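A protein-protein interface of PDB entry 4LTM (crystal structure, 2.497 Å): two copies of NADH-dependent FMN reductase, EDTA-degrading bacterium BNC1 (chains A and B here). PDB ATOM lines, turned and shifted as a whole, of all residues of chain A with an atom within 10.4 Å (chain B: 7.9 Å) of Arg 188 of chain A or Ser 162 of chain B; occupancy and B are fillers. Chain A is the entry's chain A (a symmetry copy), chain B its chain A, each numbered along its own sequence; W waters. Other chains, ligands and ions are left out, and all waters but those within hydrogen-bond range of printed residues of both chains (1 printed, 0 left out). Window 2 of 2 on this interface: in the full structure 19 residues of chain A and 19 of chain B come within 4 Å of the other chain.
ND2 of Asn 166 of chain B sits at hydrogen-bond distance from O of Pro 187 of chain A, 2.9 Å away.
O of Asp 158 of chain B is in hydrogen-bond range of OG of Ser 162 of chain B, at 3.1 Å. O of Ser 162 of chain B lies within hydrogen-bond range of ND2 of Asn 166 of chain B (2.9 Å). A ring nitrogen (ND1) of His 186 of chain A lies within hydrogen-bond range of the backbone NH (N) of Arg 188 of chain A, 2.9 Å away.
Among the printed residues, merely in contact across the chains: Gly 185 of chain A with Gln 138 of chain B, His 186 of chain A with Gln 138 of chain B, Pro 187 of chain A with Gln 163 of chain B, Arg 188 of chain A with Ser 162 of chain B, Arg 188 of chain A with Gln 163 of chain B, Arg 188 of chain A with Asn 166 of chain B and Pro 189 of chain A with Asn 166 of chain B.
Arg 188 of chain A touches just these residues of chain B: Ser 162 (3.7 Å), Gln 163 (3.95 Å) and Asn 166 (3.9 Å). Ser 162 of chain B touches just one residue of chain A: Arg 188. Of chain B, only Gln 163 (3.7 Å) and Asn 166 (2.9 Å) come within 4 Å of Pro 187 of chain A. Pro 189 of chain A touches just one residue of chain B: Asn 166 (3.1 Å). Asp 159 of chain B touches none of the printed residues of chain A. No residue of chain A comes within 4 Å of Ala 161 of chain B. Of chain A, only Pro 187 (3.7 Å) and Arg 188 (3.95 Å) come within 4 Å of Gln 163 of chain B. Asn 165 of chain B touches none of the printed residues of chain A. Asn 166 of chain B touches just these residues of chain A: Pro 187, Arg 188 and Pro 189. Printed residues of chain A within 4 Å of Gln 138 of chain B: Gly 185 and His 186. Of the printed residues of chain B, Gly 185 of chain A touches Gln 138. Printed residues of chain B within 4 Å of His 186 of chain A: Gln 138 (3.9 Å). Tyr 24 of chain B touches none of the printed residues of chain A. The nearest residue of chain A that does not touch Ser 162 of chain B is Pro 187 of chain A (4.3 Å).
Along chain A the printed residues that touch a printed residue of chain B span positions 185 to 189. Among the printed residues, no Asp or Glu carboxylate lies within 4 Å of a Lys or Arg side-chain nitrogen of the other chain.
No position is printed for both chains. Of the 8 pairs that touch across the chains among the printed residues, none has its exchanged pair printed and touching as well.
Water W1 lies within hydrogen-bond range of the backbone NH of Gly 185 of chain A (2.8 Å), the side-chain amide nitrogen of Gln 138 of chain B (3.0 Å) and the backbone carbonyl oxygen of His 186 of chain A (3.0 Å).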
ATOM      1  N   GLN A  97      33.180 -26.542  31.258  1.00  0.00           N
ATOM      2  CA  GLN A  97      33.107 -26.219  29.837  1.00  0.00           C
ATOM      3  C   GLN A  97      32.521 -24.850  29.498  1.00  0.00           C
ATOM      4  O   GLN A  97      33.052 -24.138  28.637  1.00  0.00           O
ATOM      5  CB  GLN A  97      32.356 -27.301  29.065  1.00  0.00           C
ATOM      6  CG  GLN A  97      32.365 -27.058  27.560  1.00  0.00           C
ATOM      7  CD  GLN A  97      31.723 -28.188  26.778  1.00  0.00           C
ATOM      8  OE1 GLN A  97      31.461 -29.258  27.322  1.00  0.00           O
ATOM      9  NE2 GLN A  97      31.468 -27.953  25.492  1.00  0.00           N
ATOM     10  N   PHE A  98      31.426 -24.487  30.152  1.00  0.00           N
ATOM     11  CA  PHE A  98      30.814 -23.190  29.893  1.00  0.00           C
ATOM     12  C   PHE A  98      30.855 -22.341  31.149  1.00  0.00           C
ATOM     13  O   PHE A  98      29.864 -21.721  31.530  1.00  0.00           O
ATOM     14  CB  PHE A  98      29.389 -23.356  29.368  1.00  0.00           C
ATOM     15  CG  PHE A  98      29.325 -24.034  28.032  1.00  0.00           C
ATOM     16  CD1 PHE A  98      29.752 -23.374  26.886  1.00  0.00           C
ATOM     17  CD2 PHE A  98      28.859 -25.333  27.917  1.00  0.00           C
ATOM     18  CE1 PHE A  98      29.705 -23.998  25.643  1.00  0.00           C
ATOM     19  CE2 PHE A  98      28.810 -25.964  26.681  1.00  0.00           C
ATOM     20  CZ  PHE A  98      29.236 -25.293  25.538  1.00  0.00           C
ATOM     21  N   ALA A 101      29.570 -18.560  31.399  1.00  0.00           N
ATOM     22  CA  ALA A 101      28.191 -18.198  31.068  1.00  0.00           C
ATOM     23  C   ALA A 101      27.655 -17.162  32.062  1.00  0.00           C
ATOM     24  O   ALA A 101      27.850 -17.295  33.263  1.00  0.00           O
ATOM     25  CB  ALA A 101      27.296 -19.442  31.024  1.00  0.00           C
ATOM     26  N   SER A 130      34.814 -19.507  23.991  1.00  0.00           N
ATOM     27  CA  SER A 130      34.537 -20.897  24.015  1.00  0.00           C
ATOM     28  C   SER A 130      34.027 -21.371  25.357  1.00  0.00           C
ATOM     29  O   SER A 130      33.485 -22.419  25.457  1.00  0.00           O
ATOM     30  CB  SER A 130      35.757 -21.682  23.569  1.00  0.00           C
ATOM     31  OG  SER A 130      36.541 -22.080  24.627  1.00  0.00           O
ATOM     32  N   MET A 131      34.193 -20.563  26.378  1.00  0.00           N
ATOM     33  CA  MET A 131      33.686 -20.873  27.663  1.00  0.00           C
ATOM     34  C   MET A 131      32.351 -20.237  27.910  1.00  0.00           C
ATOM     35  O   MET A 131      31.962 -20.173  29.025  1.00  0.00           O
ATOM     36  CB  MET A 131      34.688 -20.536  28.729  1.00  0.00           C
ATOM     37  CG  MET A 131      36.023 -21.166  28.436  1.00  0.00           C
ATOM     38  SD  MET A 131      37.318 -20.698  29.809  1.00  0.00           S
ATOM     39  CE  MET A 131      36.517 -21.925  31.021  1.00  0.00           C
ATOM     40  N   GLY A 132      31.682 -19.746  26.882  1.00  0.00           N
ATOM     41  CA  GLY A 132      30.348 -19.180  26.968  1.00  0.00           C
ATOM     42  C   GLY A 132      30.146 -17.829  27.618  1.00  0.00           C
ATOM     43  O   GLY A 132      29.093 -17.515  28.074  1.00  0.00           O
ATOM     44  N   ARG A 182      21.915 -14.689  33.837  1.00  0.00           N
ATOM     45  CA  ARG A 182      22.861 -15.671  34.401  1.00  0.00           C
ATOM     46  C   ARG A 182      23.372 -16.717  33.418  1.00  0.00           C
ATOM     47  O   ARG A 182      24.466 -17.247  33.584  1.00  0.00           O
ATOM     48  CB  ARG A 182      22.244 -16.392  35.604  1.00  0.00           C
ATOM     49  CG  ARG A 182      22.878 -16.011  36.925  1.00  0.00           C
ATOM     50  CD  ARG A 182      22.762 -14.502  37.167  1.00  0.00           C
ATOM     51  NE  ARG A 182      23.362 -14.094  38.437  1.00  0.00           N
ATOM     52  CZ  ARG A 182      22.820 -14.319  39.631  1.00  0.00           C
ATOM     53  NH1 ARG A 182      23.444 -13.904  40.730  1.00  0.00           N
ATOM     54  NH2 ARG A 182      21.660 -14.965  39.728  1.00  0.00           N
ATOM     55  N   HIS A 183      22.573 -17.029  32.408  1.00  0.00           N
ATOM     56  CA  HIS A 183      22.949 -18.064  31.452  1.00  0.00           C
ATOM     57  C   HIS A 183      23.326 -17.497  30.076  1.00  0.00           C
ATOM     58  O   HIS A 183      23.710 -18.250  29.185  1.00  0.00           O
ATOM     59  CB  HIS A 183      21.818 -19.095  31.315  1.00  0.00           C
ATOM     60  CG  HIS A 183      21.387 -19.704  32.619  1.00  0.00           C
ATOM     61  ND1 HIS A 183      22.280 -20.062  33.611  1.00  0.00           N
ATOM     62  CD2 HIS A 183      20.155 -20.013  33.095  1.00  0.00           C
ATOM     63  CE1 HIS A 183      21.617 -20.566  34.637  1.00  0.00           C
ATOM     64  NE2 HIS A 183      20.327 -20.548  34.349  1.00  0.00           N
ATOM     65  N   LEU A 184      23.213 -16.182  29.902  1.00  0.00           N
ATOM     66  CA  LEU A 184      23.495 -15.568  28.603  1.00  0.00           C
ATOM     67  C   LEU A 184      24.952 -15.786  28.172  1.00  0.00           C
ATOM     68  O   LEU A 184      25.887 -15.581  28.957  1.00  0.00           O
ATOM     69  CB  LEU A 184      23.151 -14.075  28.612  1.00  0.00           C
ATOM     70  CG  LEU A 184      21.669 -13.754  28.818  1.00  0.00           C
ATOM     71  CD1 LEU A 184      21.449 -12.247  28.813  1.00  0.00           C
ATOM     72  CD2 LEU A 184      20.785 -14.448  27.771  1.00  0.00           C
ATOM     73  N   GLY A 185      25.132 -16.214  26.926  1.00  0.00           N
ATOM     74  CA  GLY A 185      26.452 -16.554  26.428  1.00  0.00           C
ATOM     75  C   GLY A 185      26.558 -18.043  26.173  1.00  0.00           C
ATOM     76  O   GLY A 185      27.270 -18.487  25.272  1.00  0.00           O
ATOM     77  N   HIS A 186      25.850 -18.819  26.985  1.00  0.00           N
ATOM     78  CA  HIS A 186      25.760 -20.262  26.803  1.00  0.00           C
ATOM     79  C   HIS A 186      24.942 -20.562  25.537  1.00  0.00           C
ATOM     80  O   HIS A 186      23.902 -19.938  25.302  1.00  0.00           O
ATOM     81  CB  HIS A 186      25.084 -20.866  28.032  1.00  0.00           C
ATOM     82  CG  HIS A 186      25.286 -22.340  28.188  1.00  0.00           C
ATOM     83  ND1 HIS A 186      24.821 -23.259  27.273  1.00  0.00           N
ATOM     84  CD2 HIS A 186      25.878 -23.056  29.172  1.00  0.00           C
ATOM     85  CE1 HIS A 186      25.129 -24.478  27.680  1.00  0.00           C
ATOM     86  NE2 HIS A 186      25.771 -24.382  28.829  1.00  0.00           N
ATOM     87  N   PRO A 187      25.412 -21.505  24.709  1.00  0.00           N
ATOM     88  CA  PRO A 187      24.676 -21.883  23.492  1.00  0.00           C
ATOM     89  C   PRO A 187      23.333 -22.583  23.755  1.00  0.00           C
ATOM     90  O   PRO A 187      22.445 -22.513  22.904  1.00  0.00           O
ATOM     91  CB  PRO A 187      25.645 -22.836  22.770  1.00  0.00           C
ATOM     92  CG  PRO A 187      26.604 -23.289  23.820  1.00  0.00           C
ATOM     93  CD  PRO A 187      26.740 -22.139  24.773  1.00  0.00           C
ATOM     94  N   ARG A 188      23.194 -23.242  24.907  1.00  0.00           N
ATOM     95  CA  ARG A 188      21.978 -23.980  25.273  1.00  0.00           C
ATOM     96  C   ARG A 188      21.626 -23.748  26.746  1.00  0.00           C
ATOM     97  O   ARG A 188      21.840 -24.630  27.580  1.00  0.00           O
ATOM     98  CB  ARG A 188      22.182 -25.485  25.048  1.00  0.00           C
ATOM     99  CG  ARG A 188      22.373 -25.910  23.599  1.00  0.00           C
ATOM    100  CD  ARG A 188      21.106 -25.672  22.788  1.00  0.00           C
ATOM    101  NE  ARG A 188      19.924 -26.149  23.502  1.00  0.00           N
ATOM    102  CZ  ARG A 188      19.467 -27.398  23.443  1.00  0.00           C
ATOM    103  NH1 ARG A 188      20.092 -28.303  22.696  1.00  0.00           N
ATOM    104  NH2 ARG A 188      18.385 -27.743  24.132  1.00  0.00           N
ATOM    105  N   PRO A 189      21.143 -22.570  27.040  1.00  0.00           N
ATOM    106  CA  PRO A 189      21.021 -22.067  28.397  1.00  0.00           C
ATOM    107  C   PRO A 189      20.235 -22.949  29.346  1.00  0.00           C
ATOM    108  O   PRO A 189      20.416 -22.852  30.542  1.00  0.00           O
ATOM    109  CB  PRO A 189      20.308 -20.756  28.193  1.00  0.00           C
ATOM    110  CG  PRO A 189      20.671 -20.342  26.831  1.00  0.00           C
ATOM    111  CD  PRO A 189      20.712 -21.588  26.053  1.00  0.00           C
ATOM    112  N   SER A 190      19.381 -23.805  28.829  1.00  0.00           N
ATOM    113  CA  SER A 190      18.634 -24.696  29.683  1.00  0.00           C
ATOM    114  C   SER A 190      19.400 -25.959  30.028  1.00  0.00           C
ATOM    115  O   SER A 190      18.926 -26.746  30.810  1.00  0.00           O
ATOM    116  CB  SER A 190      17.294 -25.047  29.060  1.00  0.00           C
ATOM    117  OG  SER A 190      17.385 -26.184  28.242  1.00  0.00           O
ATOM    118  N   LEU A 191      20.564 -26.159  29.420  1.00  0.00           N
ATOM    119  CA  LEU A 191      21.466 -27.227  29.801  1.00  0.00           C
ATOM    120  C   LEU A 191      22.422 -26.707  30.854  1.00  0.00           C
ATOM    121  O   LEU A 191      23.553 -27.143  30.989  1.00  0.00           O
ATOM    122  CB  LEU A 191      22.240 -27.743  28.601  1.00  0.00           C
ATOM    123  CG  LEU A 191      21.443 -28.581  27.618  1.00  0.00           C
ATOM    124  CD1 LEU A 191      20.347 -27.739  27.052  1.00  0.00           C
ATOM    125  CD2 LEU A 191      22.299 -29.117  26.500  1.00  0.00           C
ATOM    126  N   ASP A 192      21.908 -25.754  31.603  1.00  0.00           N
ATOM    127  CA  ASP A 192      22.540 -25.188  32.752  1.00  0.00           C
ATOM    128  C   ASP A 192      23.460 -24.174  32.239  1.00  0.00           C
ATOM    129  O   ASP A 192      23.233 -23.585  31.205  1.00  0.00           O
ATOM    130  CB  ASP A 192      23.318 -26.226  33.522  1.00  0.00           C
ATOM    131  CG  ASP A 192      23.755 -25.737  34.857  1.00  0.00           C
ATOM    132  OD1 ASP A 192      23.671 -24.520  35.110  1.00  0.00           O
ATOM    133  OD2 ASP A 192      24.193 -26.577  35.664  1.00  0.00           O
ATOM    134  N   ALA A 193      24.534 -23.984  32.972  1.00  0.00           N
ATOM    135  CA  ALA A 193      25.500 -22.963  32.580  1.00  0.00           C
ATOM    136  C   ALA A 193      26.718 -22.953  33.518  1.00  0.00           C
ATOM    137  O   ALA A 193      27.655 -22.155  33.361  1.00  0.00           O
ATOM    138  CB  ALA A 193      24.829 -21.609  32.560  1.00  0.00           C
ATOM    139  N   TYR B  24      16.550 -14.003   8.332  1.00  0.00           N
ATOM    140  CA  TYR B  24      15.894 -14.725   9.415  1.00  0.00           C
ATOM    141  C   TYR B  24      16.200 -14.085  10.781  1.00  0.00           C
ATOM    142  O   TYR B  24      15.299 -13.852  11.587  1.00  0.00           O
ATOM    143  CB  TYR B  24      16.292 -16.207   9.415  1.00  0.00           C
ATOM    144  CG  TYR B  24      15.750 -16.935  10.623  1.00  0.00           C
ATOM    145  CD1 TYR B  24      14.455 -17.446  10.625  1.00  0.00           C
ATOM    146  CD2 TYR B  24      16.518 -17.084  11.775  1.00  0.00           C
ATOM    147  CE1 TYR B  24      13.944 -18.093  11.734  1.00  0.00           C
ATOM    148  CE2 TYR B  24      16.014 -17.724  12.889  1.00  0.00           C
ATOM    149  CZ  TYR B  24      14.725 -18.227  12.864  1.00  0.00           C
ATOM    150  OH  TYR B  24      14.213 -18.864  13.969  1.00  0.00           O
ATOM    151  N   GLN B 138      27.730 -14.105  21.228  1.00  0.00           N
ATOM    152  CA  GLN B 138      28.314 -15.321  20.666  1.00  0.00           C
ATOM    153  C   GLN B 138      28.149 -15.392  19.147  1.00  0.00           C
ATOM    154  O   GLN B 138      27.183 -14.876  18.588  1.00  0.00           O
ATOM    155  CB  GLN B 138      27.714 -16.582  21.299  1.00  0.00           C
ATOM    156  CG  GLN B 138      26.216 -16.724  21.098  1.00  0.00           C
ATOM    157  CD  GLN B 138      25.432 -16.319  22.336  1.00  0.00           C
ATOM    158  OE1 GLN B 138      25.719 -15.292  22.959  1.00  0.00           O
ATOM    159  NE2 GLN B 138      24.456 -17.141  22.715  1.00  0.00           N
ATOM    160  N   PHE B 140      27.450 -17.428  15.642  1.00  0.00           N
ATOM    161  CA  PHE B 140      26.756 -18.618  15.179  1.00  0.00           C
ATOM    162  C   PHE B 140      27.190 -19.002  13.778  1.00  0.00           C
ATOM    163  O   PHE B 140      27.231 -18.173  12.876  1.00  0.00           O
ATOM    164  CB  PHE B 140      25.230 -18.479  15.227  1.00  0.00           C
ATOM    165  CG  PHE B 140      24.519 -19.697  14.706  1.00  0.00           C
ATOM    166  CD1 PHE B 140      24.334 -20.805  15.518  1.00  0.00           C
ATOM    167  CD2 PHE B 140      24.087 -19.760  13.388  1.00  0.00           C
ATOM    168  CE1 PHE B 140      23.711 -21.945  15.036  1.00  0.00           C
ATOM    169  CE2 PHE B 140      23.457 -20.901  12.898  1.00  0.00           C
ATOM    170  CZ  PHE B 140      23.271 -21.995  13.728  1.00  0.00           C
ATOM    171  N   LEU B 154      12.590 -21.648   9.307  1.00  0.00           N
ATOM    172  CA  LEU B 154      13.322 -22.292  10.393  1.00  0.00           C
ATOM    173  C   LEU B 154      13.473 -23.793  10.122  1.00  0.00           C
ATOM    174  O   LEU B 154      13.651 -24.593  11.044  1.00  0.00           O
ATOM    175  CB  LEU B 154      12.628 -22.035  11.741  1.00  0.00           C
ATOM    176  CG  LEU B 154      13.416 -22.332  13.026  1.00  0.00           C
ATOM    177  CD1 LEU B 154      14.854 -21.842  12.883  1.00  0.00           C
ATOM    178  CD2 LEU B 154      12.749 -21.743  14.280  1.00  0.00           C
ATOM    179  N   VAL B 156      15.387 -26.249   9.913  1.00  0.00           N
ATOM    180  CA  VAL B 156      16.734 -26.685  10.262  1.00  0.00           C
ATOM    181  C   VAL B 156      16.672 -27.575  11.510  1.00  0.00           C
ATOM    182  O   VAL B 156      15.688 -27.541  12.252  1.00  0.00           O
ATOM    183  CB  VAL B 156      17.676 -25.467  10.486  1.00  0.00           C
ATOM    184  CG1 VAL B 156      17.388 -24.798  11.817  1.00  0.00           C
ATOM    185  CG2 VAL B 156      19.133 -25.882  10.411  1.00  0.00           C
ATOM    186  N   GLU B 157      17.711 -28.379  11.722  1.00  0.00           N
ATOM    187  CA  GLU B 157      17.785 -29.306  12.854  1.00  0.00           C
ATOM    188  C   GLU B 157      17.545 -28.633  14.208  1.00  0.00           C
ATOM    189  O   GLU B 157      17.985 -27.506  14.442  1.00  0.00           O
ATOM    190  CB  GLU B 157      19.141 -30.013  12.857  1.00  0.00           C
ATOM    191  CG  GLU B 157      19.578 -30.483  11.479  1.00  0.00           C
ATOM    192  CD  GLU B 157      20.982 -31.068  11.468  1.00  0.00           C
ATOM    193  OE1 GLU B 157      21.324 -31.764  10.484  1.00  0.00           O
ATOM    194  OE2 GLU B 157      21.744 -30.831  12.434  1.00  0.00           O
ATOM    195  N   ASP B 158      16.859 -29.345  15.097  1.00  0.00           N
ATOM    196  CA  ASP B 158      16.396 -28.796  16.371  1.00  0.00           C
ATOM    197  C   ASP B 158      17.500 -28.184  17.217  1.00  0.00           C
ATOM    198  O   ASP B 158      17.369 -27.059  17.697  1.00  0.00           O
ATOM    199  CB  ASP B 158      15.682 -29.876  17.184  1.00  0.00           C
ATOM    200  CG  ASP B 158      14.481 -30.452  16.458  1.00  0.00           C
ATOM    201  OD1 ASP B 158      14.675 -31.323  15.574  1.00  0.00           O
ATOM    202  OD2 ASP B 158      13.344 -30.032  16.773  1.00  0.00           O
ATOM    203  N   ASP B 159      18.581 -28.930  17.406  1.00  0.00           N
ATOM    204  CA  ASP B 159      19.673 -28.487  18.264  1.00  0.00           C
ATOM    205  C   ASP B 159      20.364 -27.273  17.658  1.00  0.00           C
ATOM    206  O   ASP B 159      20.756 -26.349  18.369  1.00  0.00           O
ATOM    207  CB  ASP B 159      20.674 -29.622  18.466  1.00  0.00           C
ATOM    208  CG  ASP B 159      19.994 -30.953  18.746  1.00  0.00           C
ATOM    209  OD1 ASP B 159      19.632 -31.657  17.770  1.00  0.00           O
ATOM    210  OD2 ASP B 159      19.817 -31.291  19.940  1.00  0.00           O
ATOM    211  N   VAL B 160      20.505 -27.281  16.339  1.00  0.00           N
ATOM    212  CA  VAL B 160      21.094 -26.160  15.629  1.00  0.00           C
ATOM    213  C   VAL B 160      20.190 -24.941  15.767  1.00  0.00           C
ATOM    214  O   VAL B 160      20.662 -23.827  15.992  1.00  0.00           O
ATOM    215  CB  VAL B 160      21.319 -26.503  14.140  1.00  0.00           C
ATOM    216  CG1 VAL B 160      21.663 -25.265  13.345  1.00  0.00           C
ATOM    217  CG2 VAL B 160      22.419 -27.528  14.004  1.00  0.00           C
ATOM    218  N   ALA B 161      18.886 -25.163  15.664  1.00  0.00           N
ATOM    219  CA  ALA B 161      17.925 -24.073  15.717  1.00  0.00           C
ATOM    220  C   ALA B 161      17.905 -23.415  17.091  1.00  0.00           C
ATOM    221  O   ALA B 161      17.759 -22.192  17.205  1.00  0.00           O
ATOM    222  CB  ALA B 161      16.540 -24.565  15.334  1.00  0.00           C
ATOM    223  N   SER B 162      18.052 -24.224  18.134  1.00  0.00           N
ATOM    224  CA  SER B 162      18.090 -23.694  19.492  1.00  0.00           C
ATOM    225  C   SER B 162      19.264 -22.740  19.683  1.00  0.00           C
ATOM    226  O   SER B 162      19.103 -21.664  20.255  1.00  0.00           O
ATOM    227  CB  SER B 162      18.170 -24.823  20.515  1.00  0.00           C
ATOM    228  OG  SER B 162      17.004 -25.618  20.454  1.00  0.00           O
ATOM    229  N   GLN B 163      20.433 -23.135  19.188  1.00  0.00           N
ATOM    230  CA  GLN B 163      21.638 -22.321  19.320  1.00  0.00           C
ATOM    231  C   GLN B 163      21.518 -21.006  18.581  1.00  0.00           C
ATOM    232  O   GLN B 163      21.916 -19.964  19.098  1.00  0.00           O
ATOM    233  CB  GLN B 163      22.857 -23.090  18.833  1.00  0.00           C
ATOM    234  CG  GLN B 163      23.001 -24.412  19.559  1.00  0.00           C
ATOM    235  CD  GLN B 163      24.346 -25.057  19.372  1.00  0.00           C
ATOM    236  OE1 GLN B 163      25.292 -24.427  18.892  1.00  0.00           O
ATOM    237  NE2 GLN B 163      24.446 -26.327  19.756  1.00  0.00           N
ATOM    238  N   LEU B 164      20.955 -21.061  17.377  1.00  0.00           N
ATOM    239  CA  LEU B 164      20.808 -19.875  16.563  1.00  0.00           C
ATOM    240  C   LEU B 164      19.855 -18.921  17.252  1.00  0.00           C
ATOM    241  O   LEU B 164      20.167 -17.743  17.440  1.00  0.00           O
ATOM    242  CB  LEU B 164      20.289 -20.236  15.175  1.00  0.00           C
ATOM    243  CG  LEU B 164      19.870 -19.045  14.299  1.00  0.00           C
ATOM    244  CD1 LEU B 164      21.047 -18.112  14.013  1.00  0.00           C
ATOM    245  CD2 LEU B 164      19.235 -19.532  13.007  1.00  0.00           C
ATOM    246  N   ASN B 165      18.701 -19.441  17.657  1.00  0.00           N
ATOM    247  CA  ASN B 165      17.711 -18.624  18.347  1.00  0.00           C
ATOM    248  C   ASN B 165      18.231 -18.025  19.655  1.00  0.00           C
ATOM    249  O   ASN B 165      17.930 -16.874  19.980  1.00  0.00           O
ATOM    250  CB  ASN B 165      16.413 -19.407  18.572  1.00  0.00           C
ATOM    251  CG  ASN B 165      15.678 -19.716  17.271  1.00  0.00           C
ATOM    252  OD1 ASN B 165      15.732 -18.944  16.316  1.00  0.00           O
ATOM    253  ND2 ASN B 165      15.002 -20.853  17.231  1.00  0.00           N
ATOM    254  N   ASN B 166      19.021 -18.793  20.397  1.00  0.00           N
ATOM    255  CA  ASN B 166      19.608 -18.274  21.623  1.00  0.00           C
ATOM    256  C   ASN B 166      20.584 -17.149  21.316  1.00  0.00           C
ATOM    257  O   ASN B 166      20.643 -16.152  22.038  1.00  0.00           O
ATOM    258  CB  ASN B 166      20.288 -19.387  22.427  1.00  0.00           C
ATOM    259  CG  ASN B 166      19.292 -20.395  22.972  1.00  0.00           C
ATOM    260  OD1 ASN B 166      18.138 -20.052  23.234  1.00  0.00           O
ATOM    261  ND2 ASN B 166      19.725 -21.646  23.131  1.00  0.00           N
ATOM    262  N   ALA B 167      21.333 -17.303  20.230  1.00  0.00           N
ATOM    263  CA  ALA B 167      22.282 -16.280  19.817  1.00  0.00           C
ATOM    264  C   ALA B 167      21.551 -14.982  19.453  1.00  0.00           C
ATOM    265  O   ALA B 167      21.952 -13.891  19.869  1.00  0.00           O
ATOM    266  CB  ALA B 167      23.135 -16.781  18.647  1.00  0.00           C
ATOM    267  N   ILE B 168      20.464 -15.113  18.694  1.00  0.00           N
ATOM    268  CA  ILE B 168      19.657 -13.964  18.292  1.00  0.00           C
ATOM    269  C   ILE B 168      18.934 -13.347  19.500  1.00  0.00           C
ATOM    270  O   ILE B 168      18.855 -12.124  19.610  1.00  0.00           O
ATOM    271  CB  ILE B 168      18.638 -14.326  17.172  1.00  0.00           C
ATOM    272  CG1 ILE B 168      19.323 -15.029  16.000  1.00  0.00           C
ATOM    273  CG2 ILE B 168      17.959 -13.090  16.661  1.00  0.00           C
ATOM    274  CD1 ILE B 168      18.359 -15.736  15.039  1.00  0.00           C
ATOM    275  N   ASP B 169      18.413 -14.179  20.403  1.00  0.00           N
ATOM    276  CA  ASP B 169      17.856 -13.669  21.662  1.00  0.00           C
ATOM    277  C   ASP B 169      18.881 -12.843  22.418  1.00  0.00           C
ATOM    278  O   ASP B 169      18.587 -11.737  22.885  1.00  0.00           O
ATOM    279  CB  ASP B 169      17.395 -14.801  22.586  1.00  0.00           C
ATOM    280  CG  ASP B 169      16.085 -15.439  22.140  1.00  0.00           C
ATOM    281  OD1 ASP B 169      15.257 -14.766  21.461  1.00  0.00           O
ATOM    282  OD2 ASP B 169      15.890 -16.631  22.488  1.00  0.00           O
HETATM  283  O   HOH W   1      22.991 -17.056  25.357  1.00  0.00           O
